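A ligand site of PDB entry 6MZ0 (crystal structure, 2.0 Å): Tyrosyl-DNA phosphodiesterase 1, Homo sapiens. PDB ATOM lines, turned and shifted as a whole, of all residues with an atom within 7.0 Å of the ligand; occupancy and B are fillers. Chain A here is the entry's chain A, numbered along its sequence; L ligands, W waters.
O4 of the ligand lies within salt-bridge range of NZ of Lys 118, 3.4 Å away.
The side-chain amino group (NZ) of Lys 348 is in salt-bridge range of an oxygen (O5) of the ligand.
An oxygen (O2) of the ligand sits at hydrogen-bond distance from the side-chain amide nitrogen of Asn 136 (3.2 Å).
NE2 of His 116 is in hydrogen-bond range of N2 of the ligand, 2.7 Å away.
O2 of the ligand sits at hydrogen-bond distance from NE2 of His 346 (2.6 Å).
An oxygen (O5) of the ligand is in hydrogen-bond range of the side-chain amide nitrogen (ND2) of Asn 369 (3.4 Å).
ND1 of His 346 is in hydrogen-bond range of O of Thr 134, at 2.9 Å.
N of Ser 252 sits at hydrogen-bond distance from OD1 of Asn 369 (3.1 Å).
O of Ser 367 lies within hydrogen-bond range of ND1 of His 116 (3.0 Å).
The side-chain amide oxygen of Asn 136 lies within hydrogen-bond range of the backbone NH of Cys 58, at 3.1 Å.
NZ of Lys 348 lies close to OD1 of Asn 369 (3.5 Å).
A ring nitrogen (NE2) of His 346 lies close to the side-chain carboxylate (OD2) of Asp 141 (3.5 Å).
The side-chain carboxylate (OE2) of Glu 391 sits at hydrogen-bond distance from a ring nitrogen (ND1) of His 116 (2.9 Å).
The backbone carbonyl oxygen of His 346 lies within hydrogen-bond range of the side-chain amino group of Lys 348.
Merely in contact with the ligand: Tyr 57 (3.9 Å), Ser 252 (3.8 Å), Ser 312 (3.7 Å) and Pro 314 (3.6 Å).
Hydrophobic or aromatic side chains that line the ligand: Tyr 57, His 116, Pro 314 and His 346.
Of the 25 residues printed, 10 come within 4 Å of the ligand.
The nearest printed residue that does not touch the ligand is Gly 311 (4.1 Å).
Water W6 lies within hydrogen-bond range of an oxygen (O3) of the ligand and the side-chain amide nitrogen (ND2) of Asn 369.
Water W4 lies within hydrogen-bond range of OG1 of Thr 114 (2.5 Å) and O3 of the ligand (2.7 Å).
Water W1 lies within hydrogen-bond range of an oxygen (O5) of the ligand (2.8 Å), the backbone carbonyl oxygen (O) of Ser 312 (2.8 Å) and the side-chain hydroxyl (OG) of Ser 252 (2.8 Å).
Water W3 bridges O of Gly 311 and O1 of the ligand.
Water W2 lies within hydrogen-bond range of the side-chain carboxylate (OD1) of Asp 141 (2.6 Å), the side-chain hydroxyl (OG) of Ser 312 (2.9 Å), an oxygen (O2) of the ligand (3.1 Å) and the side-chain amide nitrogen (ND2) of Asn 136 (3.5 Å).
Water W5 lies within hydrogen-bond range of the backbone carbonyl oxygen (O) of Thr 134 (2.6 Å), the side-chain amino group (NZ) of Lys 118 (3.3 Å), the side-chain amino group (NZ) of Lys 348 (3.3 Å) and an oxygen (O4) of the ligand (3.4 Å).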
ATOM      1  N   ASN A  56      13.934  -1.477   0.911  1.00  0.00           N
ATOM      2  CA  ASN A  56      14.712  -0.352   1.393  1.00  0.00           C
ATOM      3  C   ASN A  56      16.030  -0.281   0.648  1.00  0.00           C
ATOM      4  O   ASN A  56      16.313  -1.080  -0.240  1.00  0.00           O
ATOM      5  CB  ASN A  56      14.945  -0.437   2.907  1.00  0.00           C
ATOM      6  CG  ASN A  56      14.885   0.928   3.560  1.00  0.00           C
ATOM      7  OD1 ASN A  56      15.789   1.738   3.394  1.00  0.00           O
ATOM      8  ND2 ASN A  56      13.802   1.189   4.282  1.00  0.00           N
ATOM      9  N   TYR A  57      16.838   0.694   1.045  1.00  0.00           N
ATOM     10  CA  TYR A  57      18.143   0.958   0.474  1.00  0.00           C
ATOM     11  C   TYR A  57      19.266   0.497   1.383  1.00  0.00           C
ATOM     12  O   TYR A  57      20.150  -0.258   0.962  1.00  0.00           O
ATOM     13  CB  TYR A  57      18.252   2.459   0.176  1.00  0.00           C
ATOM     14  CG  TYR A  57      19.590   2.941  -0.353  1.00  0.00           C
ATOM     15  CD1 TYR A  57      20.127   2.430  -1.518  1.00  0.00           C
ATOM     16  CD2 TYR A  57      20.290   3.937   0.311  1.00  0.00           C
ATOM     17  CE1 TYR A  57      21.345   2.873  -1.999  1.00  0.00           C
ATOM     18  CE2 TYR A  57      21.505   4.396  -0.151  1.00  0.00           C
ATOM     19  CZ  TYR A  57      22.034   3.859  -1.308  1.00  0.00           C
ATOM     20  OH  TYR A  57      23.248   4.328  -1.767  1.00  0.00           O
ATOM     21  N   CYS A  58      19.235   0.910   2.646  1.00  0.00           N
ATOM     22  CA  CYS A  58      20.261   0.540   3.609  1.00  0.00           C
ATOM     23  C   CYS A  58      19.607  -0.153   4.796  1.00  0.00           C
ATOM     24  O   CYS A  58      18.541   0.263   5.269  1.00  0.00           O
ATOM     25  CB  CYS A  58      21.043   1.773   4.088  1.00  0.00           C
ATOM     26  SG  CYS A  58      22.295   1.354   5.294  1.00  0.00           S
ATOM     27  N   THR A 114      19.826   2.979  -8.081  1.00  0.00           N
ATOM     28  CA  THR A 114      19.765   2.282  -6.804  1.00  0.00           C
ATOM     29  C   THR A 114      18.335   1.830  -6.537  1.00  0.00           C
ATOM     30  O   THR A 114      17.378   2.292  -7.163  1.00  0.00           O
ATOM     31  CB  THR A 114      20.259   3.147  -5.624  1.00  0.00           C
ATOM     32  OG1 THR A 114      19.348   4.234  -5.397  1.00  0.00           O
ATOM     33  CG2 THR A 114      21.670   3.687  -5.882  1.00  0.00           C
ATOM     34  N   HIS A 116      15.903   2.482  -4.146  1.00  0.00           N
ATOM     35  CA  HIS A 116      15.769   3.542  -3.166  1.00  0.00           C
ATOM     36  C   HIS A 116      14.411   3.538  -2.466  1.00  0.00           C
ATOM     37  O   HIS A 116      14.275   4.177  -1.414  1.00  0.00           O
ATOM     38  CB  HIS A 116      16.026   4.878  -3.873  1.00  0.00           C
ATOM     39  CG  HIS A 116      16.469   5.972  -2.952  1.00  0.00           C
ATOM     40  ND1 HIS A 116      15.708   7.103  -2.730  1.00  0.00           N
ATOM     41  CD2 HIS A 116      17.593   6.114  -2.202  1.00  0.00           C
ATOM     42  CE1 HIS A 116      16.349   7.887  -1.879  1.00  0.00           C
ATOM     43  NE2 HIS A 116      17.485   7.309  -1.542  1.00  0.00           N
ATOM     44  N   LYS A 118      11.313   2.888  -0.166  1.00  0.00           N
ATOM     45  CA  LYS A 118      11.153   2.559   1.234  1.00  0.00           C
ATOM     46  C   LYS A 118       9.707   2.171   1.489  1.00  0.00           C
ATOM     47  O   LYS A 118       8.831   3.036   1.548  1.00  0.00           O
ATOM     48  CB  LYS A 118      11.600   3.720   2.105  1.00  0.00           C
ATOM     49  CG  LYS A 118      13.100   3.749   2.165  1.00  0.00           C
ATOM     50  CD  LYS A 118      13.617   5.078   1.846  1.00  0.00           C
ATOM     51  CE  LYS A 118      15.145   5.064   2.010  1.00  0.00           C
ATOM     52  NZ  LYS A 118      15.761   5.194   0.687  1.00  0.00           N
ATOM     53  N   THR A 134      10.016   7.057   4.156  1.00  0.00           N
ATOM     54  CA  THR A 134      11.241   7.656   3.654  1.00  0.00           C
ATOM     55  C   THR A 134      12.504   7.248   4.400  1.00  0.00           C
ATOM     56  O   THR A 134      13.588   7.728   4.030  1.00  0.00           O
ATOM     57  CB  THR A 134      11.115   9.203   3.663  1.00  0.00           C
ATOM     58  OG1 THR A 134      11.003   9.672   5.007  1.00  0.00           O
ATOM     59  CG2 THR A 134       9.884   9.685   2.866  1.00  0.00           C
ATOM     60  N   SER A 135      12.417   6.378   5.395  1.00  0.00           N
ATOM     61  CA  SER A 135      13.544   6.054   6.271  1.00  0.00           C
ATOM     62  C   SER A 135      14.274   4.787   5.820  1.00  0.00           C
ATOM     63  O   SER A 135      13.653   3.793   5.449  1.00  0.00           O
ATOM     64  CB  SER A 135      13.098   5.842   7.716  1.00  0.00           C
ATOM     65  OG  SER A 135      12.375   6.959   8.216  1.00  0.00           O
ATOM     66  N   ASN A 136      15.609   4.839   5.903  1.00  0.00           N
ATOM     67  CA  ASN A 136      16.407   3.616   5.852  1.00  0.00           C
ATOM     68  C   ASN A 136      16.172   2.790   7.115  1.00  0.00           C
ATOM     69  O   ASN A 136      15.715   3.297   8.124  1.00  0.00           O
ATOM     70  CB  ASN A 136      17.893   3.949   5.718  1.00  0.00           C
ATOM     71  CG  ASN A 136      18.251   4.495   4.336  1.00  0.00           C
ATOM     72  OD1 ASN A 136      18.329   3.748   3.366  1.00  0.00           O
ATOM     73  ND2 ASN A 136      18.450   5.808   4.252  1.00  0.00           N
ATOM     74  N   ILE A 138      17.884   1.748   9.618  1.00  0.00           N
ATOM     75  CA  ILE A 138      19.018   1.907  10.511  1.00  0.00           C
ATOM     76  C   ILE A 138      18.604   2.826  11.633  1.00  0.00           C
ATOM     77  O   ILE A 138      17.728   3.676  11.476  1.00  0.00           O
ATOM     78  CB  ILE A 138      20.285   2.468   9.791  1.00  0.00           C
ATOM     79  CG1 ILE A 138      20.005   3.851   9.189  1.00  0.00           C
ATOM     80  CG2 ILE A 138      20.787   1.490   8.718  1.00  0.00           C
ATOM     81  CD1 ILE A 138      21.231   4.506   8.518  1.00  0.00           C
ATOM     82  N   ASP A 141      18.146   6.737  11.246  1.00  0.00           N
ATOM     83  CA  ASP A 141      17.087   7.322  10.435  1.00  0.00           C
ATOM     84  C   ASP A 141      15.786   7.495  11.194  1.00  0.00           C
ATOM     85  O   ASP A 141      14.895   8.213  10.728  1.00  0.00           O
ATOM     86  CB  ASP A 141      16.860   6.480   9.188  1.00  0.00           C
ATOM     87  CG  ASP A 141      17.670   6.965   7.999  1.00  0.00           C
ATOM     88  OD1 ASP A 141      18.859   7.302   8.198  1.00  0.00           O
ATOM     89  OD2 ASP A 141      17.120   7.032   6.887  1.00  0.00           O
ATOM     90  N   LYS A 145      15.758  12.496  12.900  1.00  0.00           N
ATOM     91  CA  LYS A 145      15.542  13.062  11.576  1.00  0.00           C
ATOM     92  C   LYS A 145      14.051  13.348  11.374  1.00  0.00           C
ATOM     93  O   LYS A 145      13.192  12.731  12.001  1.00  0.00           O
ATOM     94  CB  LYS A 145      16.036  12.114  10.468  1.00  0.00           C
ATOM     95  CG  LYS A 145      17.549  11.772  10.581  1.00  0.00           C
ATOM     96  CD  LYS A 145      18.080  11.107   9.313  1.00  0.00           C
ATOM     97  CE  LYS A 145      19.561  10.658   9.446  1.00  0.00           C
ATOM     98  NZ  LYS A 145      20.481  11.814   9.730  1.00  0.00           N
ATOM     99  N   GLN A 147      11.240  12.499   9.089  1.00  0.00           N
ATOM    100  CA  GLN A 147      10.906  11.482   8.089  1.00  0.00           C
ATOM    101  C   GLN A 147       9.398  11.404   7.930  1.00  0.00           C
ATOM    102  O   GLN A 147       8.657  11.736   8.853  1.00  0.00           O
ATOM    103  CB  GLN A 147      11.437  10.092   8.486  1.00  0.00           C
ATOM    104  CG  GLN A 147      12.902  10.030   8.893  1.00  0.00           C
ATOM    105  CD  GLN A 147      13.784   9.537   7.739  1.00  0.00           C
ATOM    106  OE1 GLN A 147      13.416   9.652   6.555  1.00  0.00           O
ATOM    107  NE2 GLN A 147      14.941   8.961   8.081  1.00  0.00           N
ATOM    108  N   SER A 252      16.663  15.688   0.346  1.00  0.00           N
ATOM    109  CA  SER A 252      17.874  15.582   1.143  1.00  0.00           C
ATOM    110  C   SER A 252      19.090  15.190   0.308  1.00  0.00           C
ATOM    111  O   SER A 252      20.175  15.045   0.882  1.00  0.00           O
ATOM    112  CB  SER A 252      17.685  14.593   2.302  1.00  0.00           C
ATOM    113  OG  SER A 252      17.185  13.343   1.876  1.00  0.00           O
ATOM    114  N   SER A 253      18.959  15.063  -1.006  1.00  0.00           N
ATOM    115  CA  SER A 253      20.086  14.891  -1.901  1.00  0.00           C
ATOM    116  C   SER A 253      19.774  15.517  -3.250  1.00  0.00           C
ATOM    117  O   SER A 253      18.609  15.676  -3.621  1.00  0.00           O
ATOM    118  CB  SER A 253      20.468  13.419  -2.102  1.00  0.00           C
ATOM    119  OG  SER A 253      21.850  13.315  -2.384  1.00  0.00           O
ATOM    120  N   GLY A 311      26.001  13.196   7.069  1.00  0.00           N
ATOM    121  CA  GLY A 311      26.267  11.899   6.484  1.00  0.00           C
ATOM    122  C   GLY A 311      25.108  11.387   5.660  1.00  0.00           C
ATOM    123  O   GLY A 311      25.301  10.589   4.739  1.00  0.00           O
ATOM    124  N   SER A 312      23.895  11.839   5.967  1.00  0.00           N
ATOM    125  CA  SER A 312      22.698  11.446   5.221  1.00  0.00           C
ATOM    126  C   SER A 312      22.206  12.545   4.293  1.00  0.00           C
ATOM    127  O   SER A 312      21.050  12.520   3.861  1.00  0.00           O
ATOM    128  CB  SER A 312      21.591  11.036   6.175  1.00  0.00           C
ATOM    129  OG  SER A 312      22.064  10.084   7.096  1.00  0.00           O
ATOM    130  N   LEU A 313      23.059  13.524   4.006  1.00  0.00           N
ATOM    131  CA  LEU A 313      22.751  14.568   3.031  1.00  0.00           C
ATOM    132  C   LEU A 313      23.869  14.565   2.011  1.00  0.00           C
ATOM    133  O   LEU A 313      24.715  15.471   1.991  1.00  0.00           O
ATOM    134  CB  LEU A 313      22.580  15.921   3.722  1.00  0.00           C
ATOM    135  CG  LEU A 313      21.374  16.007   4.677  1.00  0.00           C
ATOM    136  CD1 LEU A 313      21.612  17.026   5.791  1.00  0.00           C
ATOM    137  CD2 LEU A 313      20.135  16.397   3.902  1.00  0.00           C
ATOM    138  N   PRO A 314      23.928  13.542   1.150  1.00  0.00           N
ATOM    139  CA  PRO A 314      25.124  13.244   0.341  1.00  0.00           C
ATOM    140  C   PRO A 314      25.272  14.068  -0.943  1.00  0.00           C
ATOM    141  O   PRO A 314      25.523  13.525  -2.020  1.00  0.00           O
ATOM    142  CB  PRO A 314      24.967  11.760   0.033  1.00  0.00           C
ATOM    143  CG  PRO A 314      23.488  11.567  -0.070  1.00  0.00           C
ATOM    144  CD  PRO A 314      22.870  12.533   0.953  1.00  0.00           C
ATOM    145  N   HIS A 346      15.053  14.021   6.168  1.00  0.00           N
ATOM    146  CA  HIS A 346      15.298  12.908   5.273  1.00  0.00           C
ATOM    147  C   HIS A 346      14.035  12.517   4.512  1.00  0.00           C
ATOM    148  O   HIS A 346      14.107  11.732   3.562  1.00  0.00           O
ATOM    149  CB  HIS A 346      15.852  11.736   6.095  1.00  0.00           C
ATOM    150  CG  HIS A 346      16.400  10.615   5.275  1.00  0.00           C
ATOM    151  ND1 HIS A 346      15.625   9.555   4.867  1.00  0.00           N
ATOM    152  CD2 HIS A 346      17.653  10.368   4.831  1.00  0.00           C
ATOM    153  CE1 HIS A 346      16.367   8.700   4.195  1.00  0.00           C
ATOM    154  NE2 HIS A 346      17.603   9.165   4.157  1.00  0.00           N
ATOM    155  N   LYS A 348      11.235  13.424   1.724  1.00  0.00           N
ATOM    156  CA  LYS A 348      11.188  14.222   0.499  1.00  0.00           C
ATOM    157  C   LYS A 348       9.734  14.479   0.161  1.00  0.00           C
ATOM    158  O   LYS A 348       8.900  13.564   0.227  1.00  0.00           O
ATOM    159  CB  LYS A 348      11.888  13.531  -0.692  1.00  0.00           C
ATOM    160  CG  LYS A 348      13.317  12.991  -0.421  1.00  0.00           C
ATOM    161  CD  LYS A 348      13.254  11.592   0.242  1.00  0.00           C
ATOM    162  CE  LYS A 348      14.573  10.855   0.175  1.00  0.00           C
ATOM    163  NZ  LYS A 348      15.452  11.195   1.294  1.00  0.00           N
ATOM    164  N   SER A 367      10.225   8.664  -1.766  1.00  0.00           N
ATOM    165  CA  SER A 367      11.650   8.447  -1.562  1.00  0.00           C
ATOM    166  C   SER A 367      12.535   9.263  -2.508  1.00  0.00           C
ATOM    167  O   SER A 367      13.754   9.310  -2.304  1.00  0.00           O
ATOM    168  CB  SER A 367      11.973   6.950  -1.755  1.00  0.00           C
ATOM    169  OG  SER A 367      11.532   6.530  -3.050  1.00  0.00           O
ATOM    170  N   ASN A 369      14.718  11.830  -4.249  1.00  0.00           N
ATOM    171  CA  ASN A 369      15.464  13.078  -4.129  1.00  0.00           C
ATOM    172  C   ASN A 369      15.411  13.850  -5.455  1.00  0.00           C
ATOM    173  O   ASN A 369      14.718  13.462  -6.408  1.00  0.00           O
ATOM    174  CB  ASN A 369      16.896  12.785  -3.673  1.00  0.00           C
ATOM    175  CG  ASN A 369      16.960  12.477  -2.211  1.00  0.00           C
ATOM    176  OD1 ASN A 369      16.372  13.199  -1.398  1.00  0.00           O
ATOM    177  ND2 ASN A 369      17.645  11.393  -1.850  1.00  0.00           N
ATOM    178  N   GLU A 391      12.023   4.011  -6.994  1.00  0.00           N
ATOM    179  CA  GLU A 391      11.538   5.035  -6.080  1.00  0.00           C
ATOM    180  C   GLU A 391      10.045   4.813  -5.889  1.00  0.00           C
ATOM    181  O   GLU A 391       9.395   4.141  -6.697  1.00  0.00           O
ATOM    182  CB  GLU A 391      11.766   6.470  -6.628  1.00  0.00           C
ATOM    183  CG  GLU A 391      13.192   6.776  -7.062  1.00  0.00           C
ATOM    184  CD  GLU A 391      14.083   7.137  -5.896  1.00  0.00           C
ATOM    185  OE1 GLU A 391      15.276   7.425  -6.134  1.00  0.00           O
ATOM    186  OE2 GLU A 391      13.616   7.113  -4.731  1.00  0.00           O
ATOM    187  N   TRP A 443      28.670  17.377   1.626  1.00  0.00           N
ATOM    188  CA  TRP A 443      29.119  16.467   2.685  1.00  0.00           C
ATOM    189  C   TRP A 443      30.603  16.159   2.649  1.00  0.00           C
ATOM    190  O   TRP A 443      31.127  15.670   3.658  1.00  0.00           O
ATOM    191  CB  TRP A 443      28.311  15.161   2.652  1.00  0.00           C
ATOM    192  CG  TRP A 443      28.675  14.158   1.603  1.00  0.00           C
ATOM    193  CD1 TRP A 443      29.259  14.388   0.397  1.00  0.00           C
ATOM    194  CD2 TRP A 443      28.441  12.744   1.680  1.00  0.00           C
ATOM    195  NE1 TRP A 443      29.415  13.200  -0.288  1.00  0.00           N
ATOM    196  CE2 TRP A 443      28.922  12.180   0.471  1.00  0.00           C
ATOM    197  CE3 TRP A 443      27.883  11.898   2.643  1.00  0.00           C
ATOM    198  CZ2 TRP A 443      28.858  10.809   0.211  1.00  0.00           C
ATOM    199  CZ3 TRP A 443      27.818  10.527   2.383  1.00  0.00           C
ATOM    200  CH2 TRP A 443      28.298  10.004   1.177  1.00  0.00           C
HETATM  201  C1  LIG L   1      19.827   8.465   0.451  1.00  0.00           C
HETATM  202  C2  LIG L   1      21.064   8.368   2.683  1.00  0.00           C
HETATM  203  C3  LIG L   1      21.021   8.348   1.159  1.00  0.00           C
HETATM  204  C4  LIG L   1      22.203   8.206  -0.818  1.00  0.00           C
HETATM  205  C5  LIG L   1      21.001   8.328  -1.517  1.00  0.00           C
HETATM  206  C6  LIG L   1      18.441   8.604   1.109  1.00  0.00           C
HETATM  207  N1  LIG L   1      22.179   8.222   0.507  1.00  0.00           N
HETATM  208  N2  LIG L   1      19.859   8.448  -0.868  1.00  0.00           N
HETATM  209  O1  LIG L   1      22.170   8.332   3.296  1.00  0.00           O
HETATM  210  O2  LIG L   1      19.996   8.418   3.336  1.00  0.00           O
HETATM  211  O3  LIG L   1      20.959   8.303  -2.903  1.00  0.00           O
HETATM  212  O4  LIG L   1      17.907   7.597   1.670  1.00  0.00           O
HETATM  213  O5  LIG L   1      17.808   9.689   1.057  1.00  0.00           O
HETATM  214  O   HOH W   1      19.518  11.812   1.637  1.00  0.00           O
HETATM  215  O   HOH W   2      20.561   7.704   6.300  1.00  0.00           O
HETATM  216  O   HOH W   3      24.784   8.982   2.491  1.00  0.00           O
HETATM  217  O   HOH W   4      19.782   6.574  -4.672  1.00  0.00           O
HETATM  218  O   HOH W   5      14.531   8.041   1.664  1.00  0.00           O
HETATM  219  O   HOH W   6      18.831   9.727  -3.707  1.00  0.00           O
